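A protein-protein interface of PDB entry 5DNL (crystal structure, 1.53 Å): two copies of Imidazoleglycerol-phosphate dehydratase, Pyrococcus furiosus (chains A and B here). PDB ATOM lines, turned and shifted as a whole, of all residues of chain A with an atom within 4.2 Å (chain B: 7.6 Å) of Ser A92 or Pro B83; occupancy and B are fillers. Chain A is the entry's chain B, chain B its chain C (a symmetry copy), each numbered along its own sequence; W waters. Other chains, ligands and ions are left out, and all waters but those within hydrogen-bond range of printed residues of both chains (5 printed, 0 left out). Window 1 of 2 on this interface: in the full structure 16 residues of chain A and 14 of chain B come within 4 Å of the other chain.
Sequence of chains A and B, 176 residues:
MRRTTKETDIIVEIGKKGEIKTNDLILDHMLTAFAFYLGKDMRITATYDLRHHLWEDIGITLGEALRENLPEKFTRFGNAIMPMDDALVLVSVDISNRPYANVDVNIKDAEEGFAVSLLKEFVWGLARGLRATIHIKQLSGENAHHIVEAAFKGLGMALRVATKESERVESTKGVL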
ATOM      1  N   PHE A  77      15.407 -16.741 -29.741  1.00  0.00           N
ATOM      2  CA  PHE A  77      14.175 -17.514 -29.710  1.00  0.00           C
ATOM      3  C   PHE A  77      13.628 -17.797 -31.084  1.00  0.00           C
ATOM      4  O   PHE A  77      13.588 -16.906 -31.940  1.00  0.00           O
ATOM      5  CB  PHE A  77      13.141 -16.747 -28.891  1.00  0.00           C
ATOM      6  CG  PHE A  77      13.499 -16.638 -27.441  1.00  0.00           C
ATOM      7  CD1 PHE A  77      13.247 -17.685 -26.578  1.00  0.00           C
ATOM      8  CD2 PHE A  77      14.102 -15.491 -26.940  1.00  0.00           C
ATOM      9  CE1 PHE A  77      13.583 -17.605 -25.245  1.00  0.00           C
ATOM     10  CE2 PHE A  77      14.451 -15.404 -25.608  1.00  0.00           C
ATOM     11  CZ  PHE A  77      14.191 -16.449 -24.755  1.00  0.00           C
ATOM     12  N   GLY A  78      13.155 -19.024 -31.312  1.00  0.00           N
ATOM     13  CA  GLY A  78      12.392 -19.324 -32.502  1.00  0.00           C
ATOM     14  C   GLY A  78      11.500 -20.522 -32.293  1.00  0.00           C
ATOM     15  O   GLY A  78      11.885 -21.450 -31.599  1.00  0.00           O
ATOM     16  N   ASN A  79      10.318 -20.484 -32.887  1.00  0.00           N
ATOM     17  CA  ASN A  79       9.361 -21.580 -32.832  1.00  0.00           C
ATOM     18  C   ASN A  79       8.892 -21.967 -34.215  1.00  0.00           C
ATOM     19  O   ASN A  79       8.975 -21.176 -35.169  1.00  0.00           O
ATOM     20  CB  ASN A  79       8.136 -21.211 -32.024  1.00  0.00           C
ATOM     21  CG  ASN A  79       8.451 -20.794 -30.617  1.00  0.00           C
ATOM     22  OD1 ASN A  79       9.152 -21.492 -29.890  1.00  0.00           O
ATOM     23  ND2 ASN A  79       7.936 -19.650 -30.221  1.00  0.00           N
ATOM     24  N   VAL A  91       7.911 -27.190 -32.345  1.00  0.00           N
ATOM     25  CA  VAL A  91       9.334 -27.106 -32.082  1.00  0.00           C
ATOM     26  C   VAL A  91       9.609 -25.737 -31.522  1.00  0.00           C
ATOM     27  O   VAL A  91       9.236 -24.727 -32.126  1.00  0.00           O
ATOM     28  CB  VAL A  91      10.194 -27.352 -33.341  1.00  0.00           C
ATOM     29  CG1 VAL A  91      11.676 -27.178 -33.015  1.00  0.00           C
ATOM     30  CG2 VAL A  91       9.893 -28.723 -33.918  1.00  0.00           C
ATOM     31  N   SER A  92      10.269 -25.694 -30.376  1.00  0.00           N
ATOM     32  CA  SER A  92      10.569 -24.432 -29.690  1.00  0.00           C
ATOM     33  C   SER A  92      12.029 -24.436 -29.285  1.00  0.00           C
ATOM     34  O   SER A  92      12.489 -25.372 -28.629  1.00  0.00           O
ATOM     35  CB  SER A  92       9.667 -24.271 -28.460  1.00  0.00           C
ATOM     36  OG  SER A  92       9.847 -23.016 -27.810  1.00  0.00           O
ATOM     37  N   VAL A  93      12.744 -23.385 -29.659  1.00  0.00           N
ATOM     38  CA  VAL A  93      14.167 -23.279 -29.438  1.00  0.00           C
ATOM     39  C   VAL A  93      14.468 -21.979 -28.699  1.00  0.00           C
ATOM     40  O   VAL A  93      13.890 -20.926 -28.985  1.00  0.00           O
ATOM     41  CB  VAL A  93      14.935 -23.293 -30.781  1.00  0.00           C
ATOM     42  CG1 VAL A  93      16.406 -22.924 -30.619  1.00  0.00           C
ATOM     43  CG2 VAL A  93      14.770 -24.635 -31.466  1.00  0.00           C
ATOM     44  N   ASP A  94      15.377 -22.063 -27.745  1.00  0.00           N
ATOM     45  CA  ASP A  94      15.954 -20.900 -27.058  1.00  0.00           C
ATOM     46  C   ASP A  94      17.463 -21.145 -27.045  1.00  0.00           C
ATOM     47  O   ASP A  94      17.933 -22.068 -26.366  1.00  0.00           O
ATOM     48  CB  ASP A  94      15.388 -20.820 -25.651  1.00  0.00           C
ATOM     49  CG  ASP A  94      16.097 -19.831 -24.770  1.00  0.00           C
ATOM     50  OD1 ASP A  94      17.035 -19.186 -25.269  1.00  0.00           O
ATOM     51  OD2 ASP A  94      15.727 -19.699 -23.563  1.00  0.00           O
ATOM     52  N   THR A 133      18.279 -24.703 -25.492  1.00  0.00           N
ATOM     53  CA  THR A 133      17.083 -25.367 -24.992  1.00  0.00           C
ATOM     54  C   THR A 133      16.226 -25.743 -26.178  1.00  0.00           C
ATOM     55  O   THR A 133      15.869 -24.862 -26.974  1.00  0.00           O
ATOM     56  CB  THR A 133      16.284 -24.360 -24.138  1.00  0.00           C
ATOM     57  OG1 THR A 133      17.123 -23.766 -23.126  1.00  0.00           O
ATOM     58  CG2 THR A 133      15.074 -24.978 -23.491  1.00  0.00           C
ATOM     59  N   ILE A 134      15.846 -27.016 -26.316  1.00  0.00           N
ATOM     60  CA  ILE A 134      15.062 -27.464 -27.450  1.00  0.00           C
ATOM     61  C   ILE A 134      13.910 -28.332 -26.994  1.00  0.00           C
ATOM     62  O   ILE A 134      14.129 -29.347 -26.341  1.00  0.00           O
ATOM     63  CB  ILE A 134      15.916 -28.243 -28.484  1.00  0.00           C
ATOM     64  CG1 ILE A 134      17.098 -27.390 -28.927  1.00  0.00           C
ATOM     65  CG2 ILE A 134      15.058 -28.640 -29.675  1.00  0.00           C
ATOM     66  CD1 ILE A 134      18.036 -28.055 -29.926  1.00  0.00           C
ATOM     67  N   HIS A 135      12.702 -27.923 -27.341  1.00  0.00           N
ATOM     68  CA  HIS A 135      11.498 -28.720 -27.124  1.00  0.00           C
ATOM     69  C   HIS A 135      10.964 -29.196 -28.454  1.00  0.00           C
ATOM     70  O   HIS A 135      10.791 -28.408 -29.385  1.00  0.00           O
ATOM     71  CB  HIS A 135      10.401 -27.903 -26.447  1.00  0.00           C
ATOM     72  CG  HIS A 135      10.651 -27.619 -25.010  1.00  0.00           C
ATOM     73  ND1 HIS A 135      10.070 -28.355 -24.003  1.00  0.00           N
ATOM     74  CD2 HIS A 135      11.416 -26.680 -24.407  1.00  0.00           C
ATOM     75  CE1 HIS A 135      10.483 -27.892 -22.839  1.00  0.00           C
ATOM     76  NE2 HIS A 135      11.295 -26.876 -23.057  1.00  0.00           N
ATOM     77  N   TYR B  37      10.842  -8.091 -23.216  1.00  0.00           N
ATOM     78  CA  TYR B  37      10.264  -8.810 -24.340  1.00  0.00           C
ATOM     79  C   TYR B  37       9.178  -8.004 -25.060  1.00  0.00           C
ATOM     80  O   TYR B  37       8.944  -8.224 -26.248  1.00  0.00           O
ATOM     81  CB  TYR B  37       9.830 -10.237 -23.907  1.00  0.00           C
ATOM     82  CG  TYR B  37      11.066 -11.078 -23.632  1.00  0.00           C
ATOM     83  CD1 TYR B  37      11.707 -11.767 -24.641  1.00  0.00           C
ATOM     84  CD2 TYR B  37      11.656 -11.086 -22.380  1.00  0.00           C
ATOM     85  CE1 TYR B  37      12.879 -12.482 -24.390  1.00  0.00           C
ATOM     86  CE2 TYR B  37      12.823 -11.788 -22.123  1.00  0.00           C
ATOM     87  CZ  TYR B  37      13.427 -12.492 -23.122  1.00  0.00           C
ATOM     88  OH  TYR B  37      14.586 -13.214 -22.870  1.00  0.00           O
ATOM     89  N   ALA B  80       2.693 -15.836 -28.222  1.00  0.00           N
ATOM     90  CA  ALA B  80       4.068 -16.250 -27.989  1.00  0.00           C
ATOM     91  C   ALA B  80       4.087 -17.648 -27.436  1.00  0.00           C
ATOM     92  O   ALA B  80       3.222 -18.012 -26.651  1.00  0.00           O
ATOM     93  CB  ALA B  80       4.768 -15.310 -27.022  1.00  0.00           C
ATOM     94  N   ILE B  81       5.087 -18.427 -27.824  1.00  0.00           N
ATOM     95  CA  ILE B  81       5.393 -19.678 -27.154  1.00  0.00           C
ATOM     96  C   ILE B  81       6.817 -19.515 -26.613  1.00  0.00           C
ATOM     97  O   ILE B  81       7.750 -19.296 -27.371  1.00  0.00           O
ATOM     98  CB  ILE B  81       5.251 -20.890 -28.073  1.00  0.00           C
ATOM     99  CG1 ILE B  81       3.767 -21.092 -28.408  1.00  0.00           C
ATOM    100  CG2 ILE B  81       5.801 -22.142 -27.365  1.00  0.00           C
ATOM    101  CD1 ILE B  81       3.557 -22.144 -29.485  1.00  0.00           C
ATOM    102  N   MET B  82       6.947 -19.586 -25.297  1.00  0.00           N
ATOM    103  CA  MET B  82       8.187 -19.321 -24.633  1.00  0.00           C
ATOM    104  C   MET B  82       8.697 -20.512 -23.850  1.00  0.00           C
ATOM    105  O   MET B  82       8.027 -20.952 -22.902  1.00  0.00           O
ATOM    106  CB  MET B  82       7.995 -18.132 -23.684  1.00  0.00           C
ATOM    107  CG  MET B  82       9.191 -17.766 -22.872  1.00  0.00           C
ATOM    108  SD  MET B  82      10.635 -17.382 -23.868  1.00  0.00           S
ATOM    109  CE  MET B  82       9.975 -16.184 -24.957  1.00  0.00           C
ATOM    110  N   PRO B  83       9.898 -21.015 -24.224  1.00  0.00           N
ATOM    111  CA  PRO B  83      10.575 -22.021 -23.422  1.00  0.00           C
ATOM    112  C   PRO B  83      11.398 -21.374 -22.327  1.00  0.00           C
ATOM    113  O   PRO B  83      11.865 -20.239 -22.484  1.00  0.00           O
ATOM    114  CB  PRO B  83      11.474 -22.729 -24.432  1.00  0.00           C
ATOM    115  CG  PRO B  83      11.773 -21.697 -25.460  1.00  0.00           C
ATOM    116  CD  PRO B  83      10.633 -20.729 -25.479  1.00  0.00           C
ATOM    117  N   MET B  84      11.553 -22.070 -21.215  1.00  0.00           N
ATOM    118  CA  MET B  84      12.618 -21.771 -20.250  1.00  0.00           C
ATOM    119  C   MET B  84      12.996 -23.085 -19.608  1.00  0.00           C
ATOM    120  O   MET B  84      12.299 -23.562 -18.715  1.00  0.00           O
ATOM    121  CB  MET B  84      12.244 -20.729 -19.205  1.00  0.00           C
ATOM    122  CG  MET B  84      13.425 -20.455 -18.264  1.00  0.00           C
ATOM    123  SD  MET B  84      13.220 -19.123 -17.088  1.00  0.00           S
ATOM    124  CE  MET B  84      12.903 -17.816 -18.262  1.00  0.00           C
ATOM    125  N   ASP B  85      14.110 -23.642 -20.064  1.00  0.00           N
ATOM    126  CA  ASP B  85      14.539 -24.979 -19.672  1.00  0.00           C
ATOM    127  C   ASP B  85      13.330 -25.937 -19.803  1.00  0.00           C
ATOM    128  O   ASP B  85      12.771 -26.041 -20.888  1.00  0.00           O
ATOM    129  CB  ASP B  85      15.177 -24.953 -18.281  1.00  0.00           C
ATOM    130  CG  ASP B  85      16.436 -24.080 -18.205  1.00  0.00           C
ATOM    131  OD1 ASP B  85      16.850 -23.449 -19.216  1.00  0.00           O
ATOM    132  OD2 ASP B  85      17.016 -24.099 -17.111  1.00  0.00           O
ATOM    133  N   ASP B  86      12.936 -26.593 -18.703  1.00  0.00           N
ATOM    134  CA  ASP B  86      11.783 -27.503 -18.699  1.00  0.00           C
ATOM    135  C   ASP B  86      10.466 -26.872 -19.105  1.00  0.00           C
ATOM    136  O   ASP B  86       9.574 -27.567 -19.607  1.00  0.00           O
ATOM    137  CB  ASP B  86      11.630 -28.155 -17.318  1.00  0.00           C
ATOM    138  CG  ASP B  86      11.514 -27.137 -16.195  1.00  0.00           C
ATOM    139  OD1 ASP B  86      12.537 -26.483 -15.905  1.00  0.00           O
ATOM    140  OD2 ASP B  86      10.406 -26.943 -15.652  1.00  0.00           O
ATOM    141  N   ALA B  87      10.296 -25.570 -18.848  1.00  0.00           N
ATOM    142  CA  ALA B  87       9.015 -24.922 -19.098  1.00  0.00           C
ATOM    143  C   ALA B  87       8.783 -24.621 -20.565  1.00  0.00           C
ATOM    144  O   ALA B  87       9.716 -24.273 -21.301  1.00  0.00           O
ATOM    145  CB  ALA B  87       8.895 -23.631 -18.288  1.00  0.00           C
ATOM    146  N   LEU B  88       7.526 -24.743 -20.973  1.00  0.00           N
ATOM    147  CA  LEU B  88       7.108 -24.312 -22.304  1.00  0.00           C
ATOM    148  C   LEU B  88       5.715 -23.757 -22.154  1.00  0.00           C
ATOM    149  O   LEU B  88       4.795 -24.486 -21.763  1.00  0.00           O
ATOM    150  CB  LEU B  88       7.138 -25.495 -23.270  1.00  0.00           C
ATOM    151  CG  LEU B  88       6.843 -25.185 -24.729  1.00  0.00           C
ATOM    152  CD1 LEU B  88       7.919 -24.296 -25.318  1.00  0.00           C
ATOM    153  CD2 LEU B  88       6.737 -26.487 -25.501  1.00  0.00           C
ATOM    154  N   VAL B  89       5.559 -22.457 -22.405  1.00  0.00           N
ATOM    155  CA  VAL B  89       4.318 -21.760 -22.090  1.00  0.00           C
ATOM    156  C   VAL B  89       3.786 -21.007 -23.297  1.00  0.00           C
ATOM    157  O   VAL B  89       4.502 -20.230 -23.920  1.00  0.00           O
ATOM    158  CB  VAL B  89       4.500 -20.794 -20.901  1.00  0.00           C
ATOM    159  CG1 VAL B  89       3.199 -20.073 -20.595  1.00  0.00           C
ATOM    160  CG2 VAL B  89       4.994 -21.535 -19.663  1.00  0.00           C
ATOM    161  N   LEU B  90       2.524 -21.250 -23.613  1.00  0.00           N
ATOM    162  CA  LEU B  90       1.831 -20.529 -24.661  1.00  0.00           C
ATOM    163  C   LEU B  90       1.100 -19.340 -24.033  1.00  0.00           C
ATOM    164  O   LEU B  90       0.369 -19.490 -23.052  1.00  0.00           O
ATOM    165  CB  LEU B  90       0.841 -21.436 -25.383  1.00  0.00           C
ATOM    166  CG  LEU B  90      -0.183 -20.765 -26.309  1.00  0.00           C
ATOM    167  CD1 LEU B  90       0.445 -20.070 -27.507  1.00  0.00           C
ATOM    168  CD2 LEU B  90      -1.222 -21.784 -26.743  1.00  0.00           C
ATOM    169  N   LEU B 139       2.349 -25.778 -21.608  1.00  0.00           N
ATOM    170  CA  LEU B 139       2.420 -26.968 -22.450  1.00  0.00           C
ATOM    171  C   LEU B 139       3.332 -28.028 -21.855  1.00  0.00           C
ATOM    172  O   LEU B 139       3.096 -29.217 -22.070  1.00  0.00           O
ATOM    173  CB  LEU B 139       2.893 -26.580 -23.857  1.00  0.00           C
ATOM    174  CG  LEU B 139       2.084 -25.458 -24.519  1.00  0.00           C
ATOM    175  CD1 LEU B 139       2.689 -25.101 -25.876  1.00  0.00           C
ATOM    176  CD2 LEU B 139       0.617 -25.857 -24.654  1.00  0.00           C
ATOM    177  N   HIS B 146      10.683 -21.062 -13.738  1.00  0.00           N
ATOM    178  CA  HIS B 146      10.752 -21.189 -15.196  1.00  0.00           C
ATOM    179  C   HIS B 146       9.380 -20.992 -15.815  1.00  0.00           C
ATOM    180  O   HIS B 146       9.237 -20.337 -16.851  1.00  0.00           O
ATOM    181  CB  HIS B 146      11.337 -22.535 -15.618  1.00  0.00           C
ATOM    182  CG  HIS B 146      12.731 -22.754 -15.146  1.00  0.00           C
ATOM    183  ND1 HIS B 146      13.304 -24.004 -15.093  1.00  0.00           N
ATOM    184  CD2 HIS B 146      13.681 -21.889 -14.737  1.00  0.00           C
ATOM    185  CE1 HIS B 146      14.547 -23.897 -14.668  1.00  0.00           C
ATOM    186  NE2 HIS B 146      14.795 -22.632 -14.424  1.00  0.00           N
ATOM    187  N   GLU B 149       8.245 -17.140 -15.149  1.00  0.00           N
ATOM    188  CA  GLU B 149       9.050 -16.219 -15.978  1.00  0.00           C
ATOM    189  C   GLU B 149       8.756 -16.411 -17.458  1.00  0.00           C
ATOM    190  O   GLU B 149       8.662 -15.432 -18.213  1.00  0.00           O
ATOM    191  CB  GLU B 149      10.526 -16.355 -15.690  1.00  0.00           C
ATOM    192  CG  GLU B 149      11.322 -15.220 -16.325  1.00  0.00           C
ATOM    193  CD  GLU B 149      12.782 -15.185 -15.934  1.00  0.00           C
ATOM    194  OE1 GLU B 149      13.190 -15.868 -14.964  1.00  0.00           O
ATOM    195  OE2 GLU B 149      13.532 -14.473 -16.640  1.00  0.00           O
ATOM    196  N   ALA B 150       8.589 -17.651 -17.906  1.00  0.00           N
ATOM    197  CA  ALA B 150       8.191 -17.880 -19.297  1.00  0.00           C
ATOM    198  C   ALA B 150       6.880 -17.183 -19.633  1.00  0.00           C
ATOM    199  O   ALA B 150       6.719 -16.606 -20.719  1.00  0.00           O
ATOM    200  CB  ALA B 150       8.122 -19.375 -19.598  1.00  0.00           C
ATOM    201  N   LYS B 153       7.672 -13.395 -19.955  1.00  0.00           N
ATOM    202  CA  LYS B 153       8.367 -13.189 -21.225  1.00  0.00           C
ATOM    203  C   LYS B 153       7.364 -13.265 -22.373  1.00  0.00           C
ATOM    204  O   LYS B 153       7.368 -12.463 -23.326  1.00  0.00           O
ATOM    205  CB  LYS B 153       9.462 -14.247 -21.459  1.00  0.00           C
ATOM    206  CG  LYS B 153      10.687 -14.171 -20.561  1.00  0.00           C
ATOM    207  CD  LYS B 153      11.752 -15.104 -21.075  1.00  0.00           C
ATOM    208  CE  LYS B 153      13.042 -15.020 -20.311  1.00  0.00           C
ATOM    209  NZ  LYS B 153      14.112 -15.769 -21.015  1.00  0.00           N
ATOM    210  N   MET B 157       6.231 -10.590 -25.282  1.00  0.00           N
ATOM    211  CA  MET B 157       6.355 -10.895 -26.712  1.00  0.00           C
ATOM    212  C   MET B 157       4.994 -10.812 -27.429  1.00  0.00           C
ATOM    213  O   MET B 157       4.878 -10.289 -28.539  1.00  0.00           O
ATOM    214  CB  MET B 157       6.995 -12.290 -26.870  1.00  0.00           C
ATOM    215  CG  MET B 157       7.591 -12.657 -28.216  1.00  0.00           C
ATOM    216  SD  MET B 157       8.448 -14.247 -28.068  1.00  0.00           S
ATOM    217  CE  MET B 157      10.089 -13.746 -27.574  1.00  0.00           C
HETATM  218  O   HOH W   1      17.603 -25.147 -21.057  1.00  0.00           O
HETATM  219  O   HOH W   2       9.906 -17.621 -28.177  1.00  0.00           O
HETATM  220  O   HOH W   3      15.829 -21.700 -21.644  1.00  0.00           O
HETATM  221  O   HOH W   4      13.918 -18.504 -21.725  1.00  0.00           O
HETATM  222  O   HOH W   5       6.965 -16.779 -29.514  1.00  0.00           O
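The side-chain amide nitrogen of Asn A79 sits at hydrogen-bond distance from the backbone carbonyl oxygen of Ile B81, at 2.9 Å.
A ring nitrogen (NE2) of His A135 lies within hydrogen-bond range of the backbone carbonyl oxygen of Asp B85.
OD1 of Asp B86 sits at hydrogen-bond distance from ND1 of His B146 (2.7 Å).
The backbone carbonyl oxygen (O) of Ser A92 is in hydrogen-bond range of the backbone NH (N) of His A135 (2.9 Å).
O of Asp A94 lies within hydrogen-bond range of N of Thr A133, 2.8 Å away.
The backbone carbonyl oxygen (O) of Val B89 lies within hydrogen-bond range of the backbone NH (N) of Met B82 (2.9 Å).
OD1 of Asn A79 is in hydrogen-bond range of OG of Ser A92 (2.7 Å).
The side-chain hydroxyl of Tyr B37 lies within hydrogen-bond range of the side-chain amino group of Lys B153 (3.2 Å).
CE2 of Phe A77 touches OH of Tyr B37, at 3.5 Å.
Phe A77 touches Met B82 (CE1 to SD, 3.3 Å).
Lys B153 touches Phe A77.
Pro B83 touches Ser A92 (CG to OG, 3.3 Å).
Ser A92 touches Leu B88 (OG to CD1, 3.4 Å).
Pro B83 touches Asp A94 (CG to CB, 3.7 Å).
Thr A133 touches Asp B85.
CD2 of His A135 touches CB of Pro B83, 3.95 Å away.
Asp B86 touches His A135.
His A135 touches Ala B87 (NE2 to O, 3.5 Å).
Of the printed residues of chain B, Ser A92 touches Pro B83 (3.3 Å) and Leu B88 (3.4 Å).
Of the printed residues of chain A, Pro B83 touches Ser A92 (3.3 Å), Asp A94 (3.7 Å) and His A135 (3.95 Å).
Of the printed residues of chain B, Thr A133 touches Asp B85 (3.6 Å).
Printed residues of chain A within 4 Å of Met B82: Phe A77 (3.3 Å).
Printed residues of chain B within 4 Å of His A135: Pro B83 (3.95 Å), Asp B85 (2.8 Å), Asp B86 (3.4 Å) and Ala B87 (3.5 Å).
Of the printed residues of chain A, Asp B86 touches His A135 (3.4 Å).
Leu B139 touches none of the printed residues of chain A.
His B146 touches none of the printed residues of chain A.
The nearest printed residue of chain A that does not touch Leu B88 is His A135 (4.04 Å).
Hydrophobic or aromatic side chains of chain B within 4 Å of the printed part of chain A: Tyr B37, Ile B81, Met B82, Pro B83 and Leu B88.
Hydrophobic or aromatic side chains of chain A within 4 Å of the printed part of chain B: Phe A77 and His A135.
No position is printed for both chains.
Of the 12 pairs that touch across the chains among the printed residues, none has its exchanged pair printed and touching as well.
Water W1 bridges the side-chain hydroxyl (OG1) of Thr A133 (2.5 Å) and the side-chain carboxylate (OD1) of Asp B85 (2.6 Å).
Water W3 lies within hydrogen-bond range of OD2 of Asp A94, OG1 of Thr A133 and N of Asp B85.
Water W4 lies within hydrogen-bond range of O of Pro B83, NZ of Lys B153 and OD2 of Asp A94.
Water W2 lies within hydrogen-bond range of the backbone carbonyl oxygen of Ile B81 (2.8 Å), the side-chain amide nitrogen of Asn A79 (3.5 Å) and the side-chain sulfur of Met B157 (3.7 Å).
Water W5 lies within hydrogen-bond range of N of Ile B81 (3.0 Å), ND2 of Asn A79 (3.1 Å) and SD of Met B157 (3.3 Å).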
